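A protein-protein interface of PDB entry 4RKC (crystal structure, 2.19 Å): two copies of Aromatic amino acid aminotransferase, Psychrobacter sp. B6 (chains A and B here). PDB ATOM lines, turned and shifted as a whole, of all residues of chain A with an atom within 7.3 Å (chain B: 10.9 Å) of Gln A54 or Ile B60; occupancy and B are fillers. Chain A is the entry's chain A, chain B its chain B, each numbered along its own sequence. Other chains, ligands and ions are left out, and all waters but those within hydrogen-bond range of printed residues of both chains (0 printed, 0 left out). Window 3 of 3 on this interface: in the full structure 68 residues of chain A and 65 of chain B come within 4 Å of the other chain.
OE2 of Glu A53 lies within salt-bridge range of NH1 of Arg B63, 2.7 Å away. ND1 of His A289 lies within hydrogen-bond range of ND1 of His B289, 3.5 Å away.
Gln A54 touches one residue of chain B. Ile B60 touches just these residues of chain A: Val A45, Lys A50, Glu A53 and Gln A54. Lys A50 touches just one residue of chain B: Ile B60. Glu A53 touches two residues of chain B. No residue of chain B comes within 4 Å of Ala A57. Asp A58 touches none of the printed residues of chain B. Of the printed residues of chain A, Ser B61 touches Val A45 (3.4 Å). Of the printed residues of chain A, His B289 touches His A289. Of the printed residues of chain B, His A289 touches His B289 (3.5 Å). Of the printed residues of chain B, Val A45 touches Ile B60 (3.9 Å), Ser B61 (3.4 Å) and Pro B62 (3.3 Å). Pro B64 touches none of the printed residues of chain A.
His B289 touches its own counterpart, His A289. Positions printed for both chains: 52, 53, 54, 55, 56, 57, 58, 59 and 289.
NE2 of His A289 lies within hydrogen-bond range of OE2 of Glu A53 (2.7 Å). NE2 of His B289 is in hydrogen-bond range of OE2 of Glu B53, 2.6 Å away. O of Pro B59 lies within hydrogen-bond range of OG of Ser B61, 3.2 Å away. The backbone carbonyl oxygen of Ser B61 is in hydrogen-bond range of the guanidinium group of Arg B63, 2.6 Å away.
Of the 16 printed residues of chain A, 5 touch a printed residue of chain B. Hydrophobic or aromatic side chains of chain A that line the printed part of chain B: Val A45 and His A289.
Among the printed residues, pairs that only touch across the chains: Val A45 with Ile B60, Val A45 with Ser B61, Val A45 with Pro B62, Lys A50 with Ile B60, Glu A53 with Ile B60 and Gln A54 with Ile B60.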
ATOM      1  N   VAL A  45       9.076  21.071  -6.676  1.00  0.00           N
ATOM      2  CA  VAL A  45       9.912  19.935  -6.429  1.00  0.00           C
ATOM      3  C   VAL A  45      11.290  20.545  -6.265  1.00  0.00           C
ATOM      4  O   VAL A  45      11.826  21.128  -7.207  1.00  0.00           O
ATOM      5  CB  VAL A  45       9.860  18.932  -7.563  1.00  0.00           C
ATOM      6  CG1 VAL A  45      11.006  17.918  -7.433  1.00  0.00           C
ATOM      7  CG2 VAL A  45       8.500  18.211  -7.557  1.00  0.00           C
ATOM      8  N   LEU A  46      11.865  20.470  -5.074  1.00  0.00           N
ATOM      9  CA  LEU A  46      13.204  21.119  -4.856  1.00  0.00           C
ATOM     10  C   LEU A  46      14.284  20.475  -5.706  1.00  0.00           C
ATOM     11  O   LEU A  46      14.276  19.299  -5.897  1.00  0.00           O
ATOM     12  CB  LEU A  46      13.658  21.119  -3.368  1.00  0.00           C
ATOM     13  CG  LEU A  46      12.641  21.729  -2.376  1.00  0.00           C
ATOM     14  CD1 LEU A  46      13.286  21.999  -1.024  1.00  0.00           C
ATOM     15  CD2 LEU A  46      12.080  23.002  -2.934  1.00  0.00           C
ATOM     16  N   ASP A  47      15.245  21.261  -6.179  1.00  0.00           N
ATOM     17  CA  ASP A  47      16.301  20.702  -7.026  1.00  0.00           C
ATOM     18  C   ASP A  47      17.110  19.746  -6.226  1.00  0.00           C
ATOM     19  O   ASP A  47      17.567  18.755  -6.734  1.00  0.00           O
ATOM     20  CB  ASP A  47      17.245  21.815  -7.571  1.00  0.00           C
ATOM     21  CG  ASP A  47      16.585  22.648  -8.666  1.00  0.00           C
ATOM     22  OD1 ASP A  47      15.548  22.151  -9.262  1.00  0.00           O
ATOM     23  OD2 ASP A  47      17.093  23.779  -8.943  1.00  0.00           O
ATOM     24  N   CYS A  48      17.338  20.054  -4.955  1.00  0.00           N
ATOM     25  CA  CYS A  48      18.159  19.173  -4.144  1.00  0.00           C
ATOM     26  C   CYS A  48      17.449  17.811  -3.976  1.00  0.00           C
ATOM     27  O   CYS A  48      18.099  16.768  -3.926  1.00  0.00           O
ATOM     28  CB  CYS A  48      18.475  19.807  -2.790  1.00  0.00           C
ATOM     29  SG  CYS A  48      17.012  20.399  -1.903  1.00  0.00           S
ATOM     30  N   VAL A  49      16.131  17.858  -3.838  1.00  0.00           N
ATOM     31  CA  VAL A  49      15.299  16.655  -3.556  1.00  0.00           C
ATOM     32  C   VAL A  49      15.324  15.824  -4.803  1.00  0.00           C
ATOM     33  O   VAL A  49      15.494  14.602  -4.734  1.00  0.00           O
ATOM     34  CB  VAL A  49      13.871  17.067  -3.105  1.00  0.00           C
ATOM     35  CG1 VAL A  49      12.865  15.969  -3.299  1.00  0.00           C
ATOM     36  CG2 VAL A  49      13.910  17.558  -1.640  1.00  0.00           C
ATOM     37  N   LYS A  50      15.227  16.531  -5.929  1.00  0.00           N
ATOM     38  CA  LYS A  50      15.250  15.945  -7.255  1.00  0.00           C
ATOM     39  C   LYS A  50      16.542  15.167  -7.459  1.00  0.00           C
ATOM     40  O   LYS A  50      16.466  14.028  -7.861  1.00  0.00           O
ATOM     41  CB  LYS A  50      15.059  17.079  -8.288  1.00  0.00           C
ATOM     42  CG  LYS A  50      14.941  16.689  -9.741  1.00  0.00           C
ATOM     43  CD  LYS A  50      14.495  17.884 -10.595  1.00  0.00           C
ATOM     44  CE  LYS A  50      13.998  17.469 -11.958  1.00  0.00           C
ATOM     45  NZ  LYS A  50      15.139  17.249 -12.902  1.00  0.00           N
ATOM     46  N   ILE A  51      17.713  15.757  -7.146  1.00  0.00           N
ATOM     47  CA  ILE A  51      18.971  15.023  -7.231  1.00  0.00           C
ATOM     48  C   ILE A  51      18.985  13.810  -6.287  1.00  0.00           C
ATOM     49  O   ILE A  51      19.487  12.752  -6.634  1.00  0.00           O
ATOM     50  CB  ILE A  51      20.179  15.943  -6.917  1.00  0.00           C
ATOM     51  CG1 ILE A  51      20.374  16.871  -8.147  1.00  0.00           C
ATOM     52  CG2 ILE A  51      21.458  15.139  -6.690  1.00  0.00           C
ATOM     53  CD1 ILE A  51      20.845  18.271  -7.865  1.00  0.00           C
ATOM     54  N   ALA A  52      18.485  14.004  -5.063  1.00  0.00           N
ATOM     55  CA  ALA A  52      18.500  12.957  -4.023  1.00  0.00           C
ATOM     56  C   ALA A  52      17.694  11.774  -4.532  1.00  0.00           C
ATOM     57  O   ALA A  52      18.124  10.648  -4.416  1.00  0.00           O
ATOM     58  CB  ALA A  52      17.875  13.486  -2.758  1.00  0.00           C
ATOM     59  N   GLU A  53      16.559  12.066  -5.164  1.00  0.00           N
ATOM     60  CA  GLU A  53      15.654  11.005  -5.651  1.00  0.00           C
ATOM     61  C   GLU A  53      16.201  10.337  -6.906  1.00  0.00           C
ATOM     62  O   GLU A  53      16.077   9.108  -7.076  1.00  0.00           O
ATOM     63  CB  GLU A  53      14.276  11.615  -5.865  1.00  0.00           C
ATOM     64  CG  GLU A  53      13.583  11.862  -4.507  1.00  0.00           C
ATOM     65  CD  GLU A  53      12.117  12.230  -4.633  1.00  0.00           C
ATOM     66  OE1 GLU A  53      11.766  13.095  -5.480  1.00  0.00           O
ATOM     67  OE2 GLU A  53      11.313  11.727  -3.842  1.00  0.00           O
ATOM     68  N   GLN A  54      16.890  11.105  -7.759  1.00  0.00           N
ATOM     69  CA  GLN A  54      17.594  10.443  -8.826  1.00  0.00           C
ATOM     70  C   GLN A  54      18.588   9.450  -8.224  1.00  0.00           C
ATOM     71  O   GLN A  54      18.750   8.366  -8.701  1.00  0.00           O
ATOM     72  CB  GLN A  54      18.293  11.467  -9.780  1.00  0.00           C
ATOM     73  CG  GLN A  54      17.235  12.341 -10.459  1.00  0.00           C
ATOM     74  CD  GLN A  54      17.792  13.659 -11.039  1.00  0.00           C
ATOM     75  OE1 GLN A  54      18.959  14.022 -10.792  1.00  0.00           O
ATOM     76  NE2 GLN A  54      16.956  14.353 -11.847  1.00  0.00           N
ATOM     77  N   ARG A  55      19.324   9.841  -7.205  1.00  0.00           N
ATOM     78  CA  ARG A  55      20.252   8.887  -6.540  1.00  0.00           C
ATOM     79  C   ARG A  55      19.532   7.662  -5.941  1.00  0.00           C
ATOM     80  O   ARG A  55      20.001   6.532  -6.013  1.00  0.00           O
ATOM     81  CB  ARG A  55      21.051   9.632  -5.490  1.00  0.00           C
ATOM     82  CG  ARG A  55      21.910  10.775  -6.077  1.00  0.00           C
ATOM     83  CD  ARG A  55      22.812  11.355  -4.973  1.00  0.00           C
ATOM     84  NE  ARG A  55      23.563  12.559  -5.400  1.00  0.00           N
ATOM     85  CZ  ARG A  55      24.314  13.320  -4.580  1.00  0.00           C
ATOM     86  NH1 ARG A  55      24.392  13.053  -3.253  1.00  0.00           N
ATOM     87  NH2 ARG A  55      24.921  14.386  -5.079  1.00  0.00           N
ATOM     88  N   ILE A  56      18.383   7.890  -5.321  1.00  0.00           N
ATOM     89  CA  ILE A  56      17.647   6.799  -4.711  1.00  0.00           C
ATOM     90  C   ILE A  56      17.175   5.833  -5.830  1.00  0.00           C
ATOM     91  O   ILE A  56      17.198   4.608  -5.679  1.00  0.00           O
ATOM     92  CB  ILE A  56      16.476   7.342  -3.848  1.00  0.00           C
ATOM     93  CG1 ILE A  56      17.080   8.028  -2.635  1.00  0.00           C
ATOM     94  CG2 ILE A  56      15.500   6.182  -3.469  1.00  0.00           C
ATOM     95  CD1 ILE A  56      16.225   9.110  -1.976  1.00  0.00           C
ATOM     96  N   ALA A  57      16.840   6.419  -6.966  1.00  0.00           N
ATOM     97  CA  ALA A  57      16.207   5.708  -8.143  1.00  0.00           C
ATOM     98  C   ALA A  57      17.259   4.958  -8.963  1.00  0.00           C
ATOM     99  O   ALA A  57      16.948   4.234  -9.891  1.00  0.00           O
ATOM    100  CB  ALA A  57      15.500   6.721  -8.999  1.00  0.00           C
ATOM    101  N   ASP A  58      18.520   5.093  -8.601  1.00  0.00           N
ATOM    102  CA  ASP A  58      19.560   4.481  -9.405  1.00  0.00           C
ATOM    103  C   ASP A  58      20.754   4.032  -8.567  1.00  0.00           C
ATOM    104  O   ASP A  58      21.589   4.840  -8.296  1.00  0.00           O
ATOM    105  CB  ASP A  58      20.073   5.458 -10.479  1.00  0.00           C
ATOM    106  CG  ASP A  58      21.400   4.977 -11.100  1.00  0.00           C
ATOM    107  OD1 ASP A  58      21.341   3.923 -11.802  1.00  0.00           O
ATOM    108  OD2 ASP A  58      22.482   5.602 -10.820  1.00  0.00           O
ATOM    109  N   PRO A  59      20.857   2.743  -8.234  1.00  0.00           N
ATOM    110  CA  PRO A  59      19.876   1.664  -8.622  1.00  0.00           C
ATOM    111  C   PRO A  59      18.645   1.629  -7.711  1.00  0.00           C
ATOM    112  O   PRO A  59      18.747   2.052  -6.585  1.00  0.00           O
ATOM    113  CB  PRO A  59      20.670   0.366  -8.414  1.00  0.00           C
ATOM    114  CG  PRO A  59      21.642   0.734  -7.275  1.00  0.00           C
ATOM    115  CD  PRO A  59      21.866   2.271  -7.283  1.00  0.00           C
ATOM    116  N   HIS A 289      11.753   5.869   1.987  1.00  0.00           N
ATOM    117  CA  HIS A 289      12.007   6.742   0.878  1.00  0.00           C
ATOM    118  C   HIS A 289      12.276   8.170   1.341  1.00  0.00           C
ATOM    119  O   HIS A 289      13.235   8.817   0.866  1.00  0.00           O
ATOM    120  CB  HIS A 289      10.920   6.711  -0.185  1.00  0.00           C
ATOM    121  CG  HIS A 289      11.251   7.595  -1.333  1.00  0.00           C
ATOM    122  ND1 HIS A 289      11.996   7.160  -2.412  1.00  0.00           N
ATOM    123  CD2 HIS A 289      11.037   8.917  -1.529  1.00  0.00           C
ATOM    124  CE1 HIS A 289      12.145   8.158  -3.275  1.00  0.00           C
ATOM    125  NE2 HIS A 289      11.593   9.243  -2.752  1.00  0.00           N
ATOM    126  N   ALA B  52       7.336   0.114 -11.151  1.00  0.00           N
ATOM    127  CA  ALA B  52       6.498   1.076 -10.510  1.00  0.00           C
ATOM    128  C   ALA B  52       7.387   2.296 -10.098  1.00  0.00           C
ATOM    129  O   ALA B  52       7.027   3.458 -10.254  1.00  0.00           O
ATOM    130  CB  ALA B  52       5.865   0.380  -9.269  1.00  0.00           C
ATOM    131  N   GLU B  53       8.556   2.012  -9.548  1.00  0.00           N
ATOM    132  CA  GLU B  53       9.398   3.085  -9.022  1.00  0.00           C
ATOM    133  C   GLU B  53      10.027   3.817 -10.153  1.00  0.00           C
ATOM    134  O   GLU B  53      10.358   4.969  -9.966  1.00  0.00           O
ATOM    135  CB  GLU B  53      10.449   2.576  -8.025  1.00  0.00           C
ATOM    136  CG  GLU B  53       9.774   1.994  -6.797  1.00  0.00           C
ATOM    137  CD  GLU B  53      10.761   1.677  -5.706  1.00  0.00           C
ATOM    138  OE1 GLU B  53      11.799   1.016  -5.923  1.00  0.00           O
ATOM    139  OE2 GLU B  53      10.486   2.041  -4.581  1.00  0.00           O
ATOM    140  N   GLN B  54      10.237   3.188 -11.293  1.00  0.00           N
ATOM    141  CA  GLN B  54      10.765   3.980 -12.435  1.00  0.00           C
ATOM    142  C   GLN B  54       9.705   4.970 -12.912  1.00  0.00           C
ATOM    143  O   GLN B  54      10.008   6.068 -13.345  1.00  0.00           O
ATOM    144  CB  GLN B  54      11.124   3.095 -13.636  1.00  0.00           C
ATOM    145  CG  GLN B  54      12.426   2.363 -13.510  1.00  0.00           C
ATOM    146  CD  GLN B  54      12.448   1.102 -14.382  1.00  0.00           C
ATOM    147  OE1 GLN B  54      11.505   0.828 -15.161  1.00  0.00           O
ATOM    148  NE2 GLN B  54      13.508   0.319 -14.245  1.00  0.00           N
ATOM    149  N   ARG B  55       8.452   4.551 -12.825  1.00  0.00           N
ATOM    150  CA  ARG B  55       7.315   5.402 -13.154  1.00  0.00           C
ATOM    151  C   ARG B  55       7.172   6.550 -12.154  1.00  0.00           C
ATOM    152  O   ARG B  55       7.003   7.704 -12.522  1.00  0.00           O
ATOM    153  CB  ARG B  55       6.048   4.538 -13.154  1.00  0.00           C
ATOM    154  CG  ARG B  55       5.896   3.772 -14.447  1.00  0.00           C
ATOM    155  CD  ARG B  55       4.604   3.016 -14.455  1.00  0.00           C
ATOM    156  NE  ARG B  55       4.697   1.896 -15.407  1.00  0.00           N
ATOM    157  CZ  ARG B  55       3.723   0.994 -15.595  1.00  0.00           C
ATOM    158  NH1 ARG B  55       2.576   1.088 -14.895  1.00  0.00           N
ATOM    159  NH2 ARG B  55       3.893   0.011 -16.481  1.00  0.00           N
ATOM    160  N   ILE B  56       7.289   6.222 -10.864  1.00  0.00           N
ATOM    161  CA  ILE B  56       7.354   7.290  -9.846  1.00  0.00           C
ATOM    162  C   ILE B  56       8.492   8.310 -10.091  1.00  0.00           C
ATOM    163  O   ILE B  56       8.339   9.510  -9.778  1.00  0.00           O
ATOM    164  CB  ILE B  56       7.446   6.679  -8.411  1.00  0.00           C
ATOM    165  CG1 ILE B  56       6.119   5.978  -8.111  1.00  0.00           C
ATOM    166  CG2 ILE B  56       7.845   7.779  -7.406  1.00  0.00           C
ATOM    167  CD1 ILE B  56       6.080   4.824  -7.119  1.00  0.00           C
ATOM    168  N   ALA B  57       9.635   7.853 -10.599  1.00  0.00           N
ATOM    169  CA  ALA B  57      10.778   8.770 -10.856  1.00  0.00           C
ATOM    170  C   ALA B  57      10.731   9.433 -12.217  1.00  0.00           C
ATOM    171  O   ALA B  57      11.706  10.126 -12.615  1.00  0.00           O
ATOM    172  CB  ALA B  57      12.078   8.021 -10.753  1.00  0.00           C
ATOM    173  N   ASP B  58       9.681   9.154 -12.977  1.00  0.00           N
ATOM    174  CA  ASP B  58       9.608   9.697 -14.343  1.00  0.00           C
ATOM    175  C   ASP B  58       8.207  10.142 -14.689  1.00  0.00           C
ATOM    176  O   ASP B  58       7.464   9.358 -15.237  1.00  0.00           O
ATOM    177  CB  ASP B  58      10.060   8.663 -15.375  1.00  0.00           C
ATOM    178  CG  ASP B  58       9.873   9.151 -16.822  1.00  0.00           C
ATOM    179  OD1 ASP B  58      10.749   9.932 -17.278  1.00  0.00           O
ATOM    180  OD2 ASP B  58       8.854   8.753 -17.473  1.00  0.00           O
ATOM    181  N   PRO B  59       7.857  11.408 -14.416  1.00  0.00           N
ATOM    182  CA  PRO B  59       8.743  12.396 -13.777  1.00  0.00           C
ATOM    183  C   PRO B  59       8.702  12.374 -12.225  1.00  0.00           C
ATOM    184  O   PRO B  59       7.738  11.888 -11.655  1.00  0.00           O
ATOM    185  CB  PRO B  59       8.179  13.725 -14.258  1.00  0.00           C
ATOM    186  CG  PRO B  59       6.698  13.427 -14.504  1.00  0.00           C
ATOM    187  CD  PRO B  59       6.481  11.920 -14.537  1.00  0.00           C
ATOM    188  N   ILE B  60       9.751  12.916 -11.604  1.00  0.00           N
ATOM    189  CA  ILE B  60       9.778  13.170 -10.188  1.00  0.00           C
ATOM    190  C   ILE B  60       8.702  14.244  -9.915  1.00  0.00           C
ATOM    191  O   ILE B  60       8.674  15.289 -10.584  1.00  0.00           O
ATOM    192  CB  ILE B  60      11.211  13.534  -9.687  1.00  0.00           C
ATOM    193  CG1 ILE B  60      12.049  12.230  -9.617  1.00  0.00           C
ATOM    194  CG2 ILE B  60      11.151  14.156  -8.292  1.00  0.00           C
ATOM    195  CD1 ILE B  60      13.557  12.401  -9.570  1.00  0.00           C
ATOM    196  N   SER B  61       7.748  13.922  -9.032  1.00  0.00           N
ATOM    197  CA  SER B  61       6.562  14.744  -8.923  1.00  0.00           C
ATOM    198  C   SER B  61       6.518  15.505  -7.599  1.00  0.00           C
ATOM    199  O   SER B  61       7.173  15.046  -6.610  1.00  0.00           O
ATOM    200  CB  SER B  61       5.248  13.923  -9.092  1.00  0.00           C
ATOM    201  OG  SER B  61       5.241  13.328 -10.376  1.00  0.00           O
ATOM    202  N   PRO B  62       5.678  16.594  -7.559  1.00  0.00           N
ATOM    203  CA  PRO B  62       5.322  17.239  -6.322  1.00  0.00           C
ATOM    204  C   PRO B  62       4.786  16.218  -5.356  1.00  0.00           C
ATOM    205  O   PRO B  62       4.291  15.163  -5.762  1.00  0.00           O
ATOM    206  CB  PRO B  62       4.196  18.157  -6.709  1.00  0.00           C
ATOM    207  CG  PRO B  62       4.425  18.496  -8.112  1.00  0.00           C
ATOM    208  CD  PRO B  62       4.944  17.185  -8.697  1.00  0.00           C
ATOM    209  N   ARG B  63       4.912  16.524  -4.064  1.00  0.00           N
ATOM    210  CA  ARG B  63       4.725  15.549  -3.030  1.00  0.00           C
ATOM    211  C   ARG B  63       3.734  16.091  -2.033  1.00  0.00           C
ATOM    212  O   ARG B  63       4.061  16.265  -0.834  1.00  0.00           O
ATOM    213  CB  ARG B  63       6.059  15.089  -2.405  1.00  0.00           C
ATOM    214  CG  ARG B  63       6.056  13.570  -2.165  1.00  0.00           C
ATOM    215  CD  ARG B  63       6.019  12.742  -3.461  1.00  0.00           C
ATOM    216  NE  ARG B  63       6.949  13.298  -4.441  1.00  0.00           N
ATOM    217  CZ  ARG B  63       8.270  13.175  -4.378  1.00  0.00           C
ATOM    218  NH1 ARG B  63       8.816  12.493  -3.383  1.00  0.00           N
ATOM    219  NH2 ARG B  63       9.056  13.801  -5.284  1.00  0.00           N
ATOM    220  N   PRO B  64       2.485  16.346  -2.540  1.00  0.00           N
ATOM    221  CA  PRO B  64       1.439  16.789  -1.590  1.00  0.00           C
ATOM    222  C   PRO B  64       1.116  15.667  -0.584  1.00  0.00           C
ATOM    223  O   PRO B  64       1.422  14.505  -0.845  1.00  0.00           O
ATOM    224  CB  PRO B  64       0.223  17.094  -2.513  1.00  0.00           C
ATOM    225  CG  PRO B  64       0.458  16.142  -3.712  1.00  0.00           C
ATOM    226  CD  PRO B  64       1.980  16.252  -3.928  1.00  0.00           C
ATOM    227  N   SER B 288       3.764   8.729   0.746  1.00  0.00           N
ATOM    228  CA  SER B 288       3.463   8.787  -0.666  1.00  0.00           C
ATOM    229  C   SER B 288       4.244   7.745  -1.464  1.00  0.00           C
ATOM    230  O   SER B 288       3.719   7.081  -2.371  1.00  0.00           O
ATOM    231  CB  SER B 288       3.896  10.181  -1.177  1.00  0.00           C
ATOM    232  OG  SER B 288       3.814  10.166  -2.579  1.00  0.00           O
ATOM    233  N   HIS B 289       5.561   7.662  -1.213  1.00  0.00           N
ATOM    234  CA  HIS B 289       6.301   6.692  -2.036  1.00  0.00           C
ATOM    235  C   HIS B 289       5.747   5.246  -2.047  1.00  0.00           C
ATOM    236  O   HIS B 289       5.451   4.663  -3.150  1.00  0.00           O
ATOM    237  CB  HIS B 289       7.806   6.665  -1.757  1.00  0.00           C
ATOM    238  CG  HIS B 289       8.529   5.893  -2.800  1.00  0.00           C
ATOM    239  ND1 HIS B 289       8.971   6.466  -3.981  1.00  0.00           N
ATOM    240  CD2 HIS B 289       8.801   4.560  -2.885  1.00  0.00           C
ATOM    241  CE1 HIS B 289       9.507   5.520  -4.745  1.00  0.00           C
ATOM    242  NE2 HIS B 289       9.445   4.359  -4.087  1.00  0.00           N
ATOM    243  N   ARG B 292       2.202   5.055  -3.655  1.00  0.00           N
ATOM    244  CA  ARG B 292       2.245   4.972  -5.131  1.00  0.00           C
ATOM    245  C   ARG B 292       2.727   3.660  -5.655  1.00  0.00           C
ATOM    246  O   ARG B 292       2.220   3.182  -6.654  1.00  0.00           O
ATOM    247  CB  ARG B 292       3.152   6.075  -5.702  1.00  0.00           C
ATOM    248  CG  ARG B 292       2.451   7.392  -5.619  1.00  0.00           C
ATOM    249  CD  ARG B 292       3.117   8.350  -6.559  1.00  0.00           C
ATOM    250  NE  ARG B 292       2.740   8.040  -7.922  1.00  0.00           N
ATOM    251  CZ  ARG B 292       3.344   8.507  -9.000  1.00  0.00           C
ATOM    252  NH1 ARG B 292       4.373   9.332  -8.919  1.00  0.00           N
ATOM    253  NH2 ARG B 292       2.874   8.152 -10.172  1.00  0.00           N
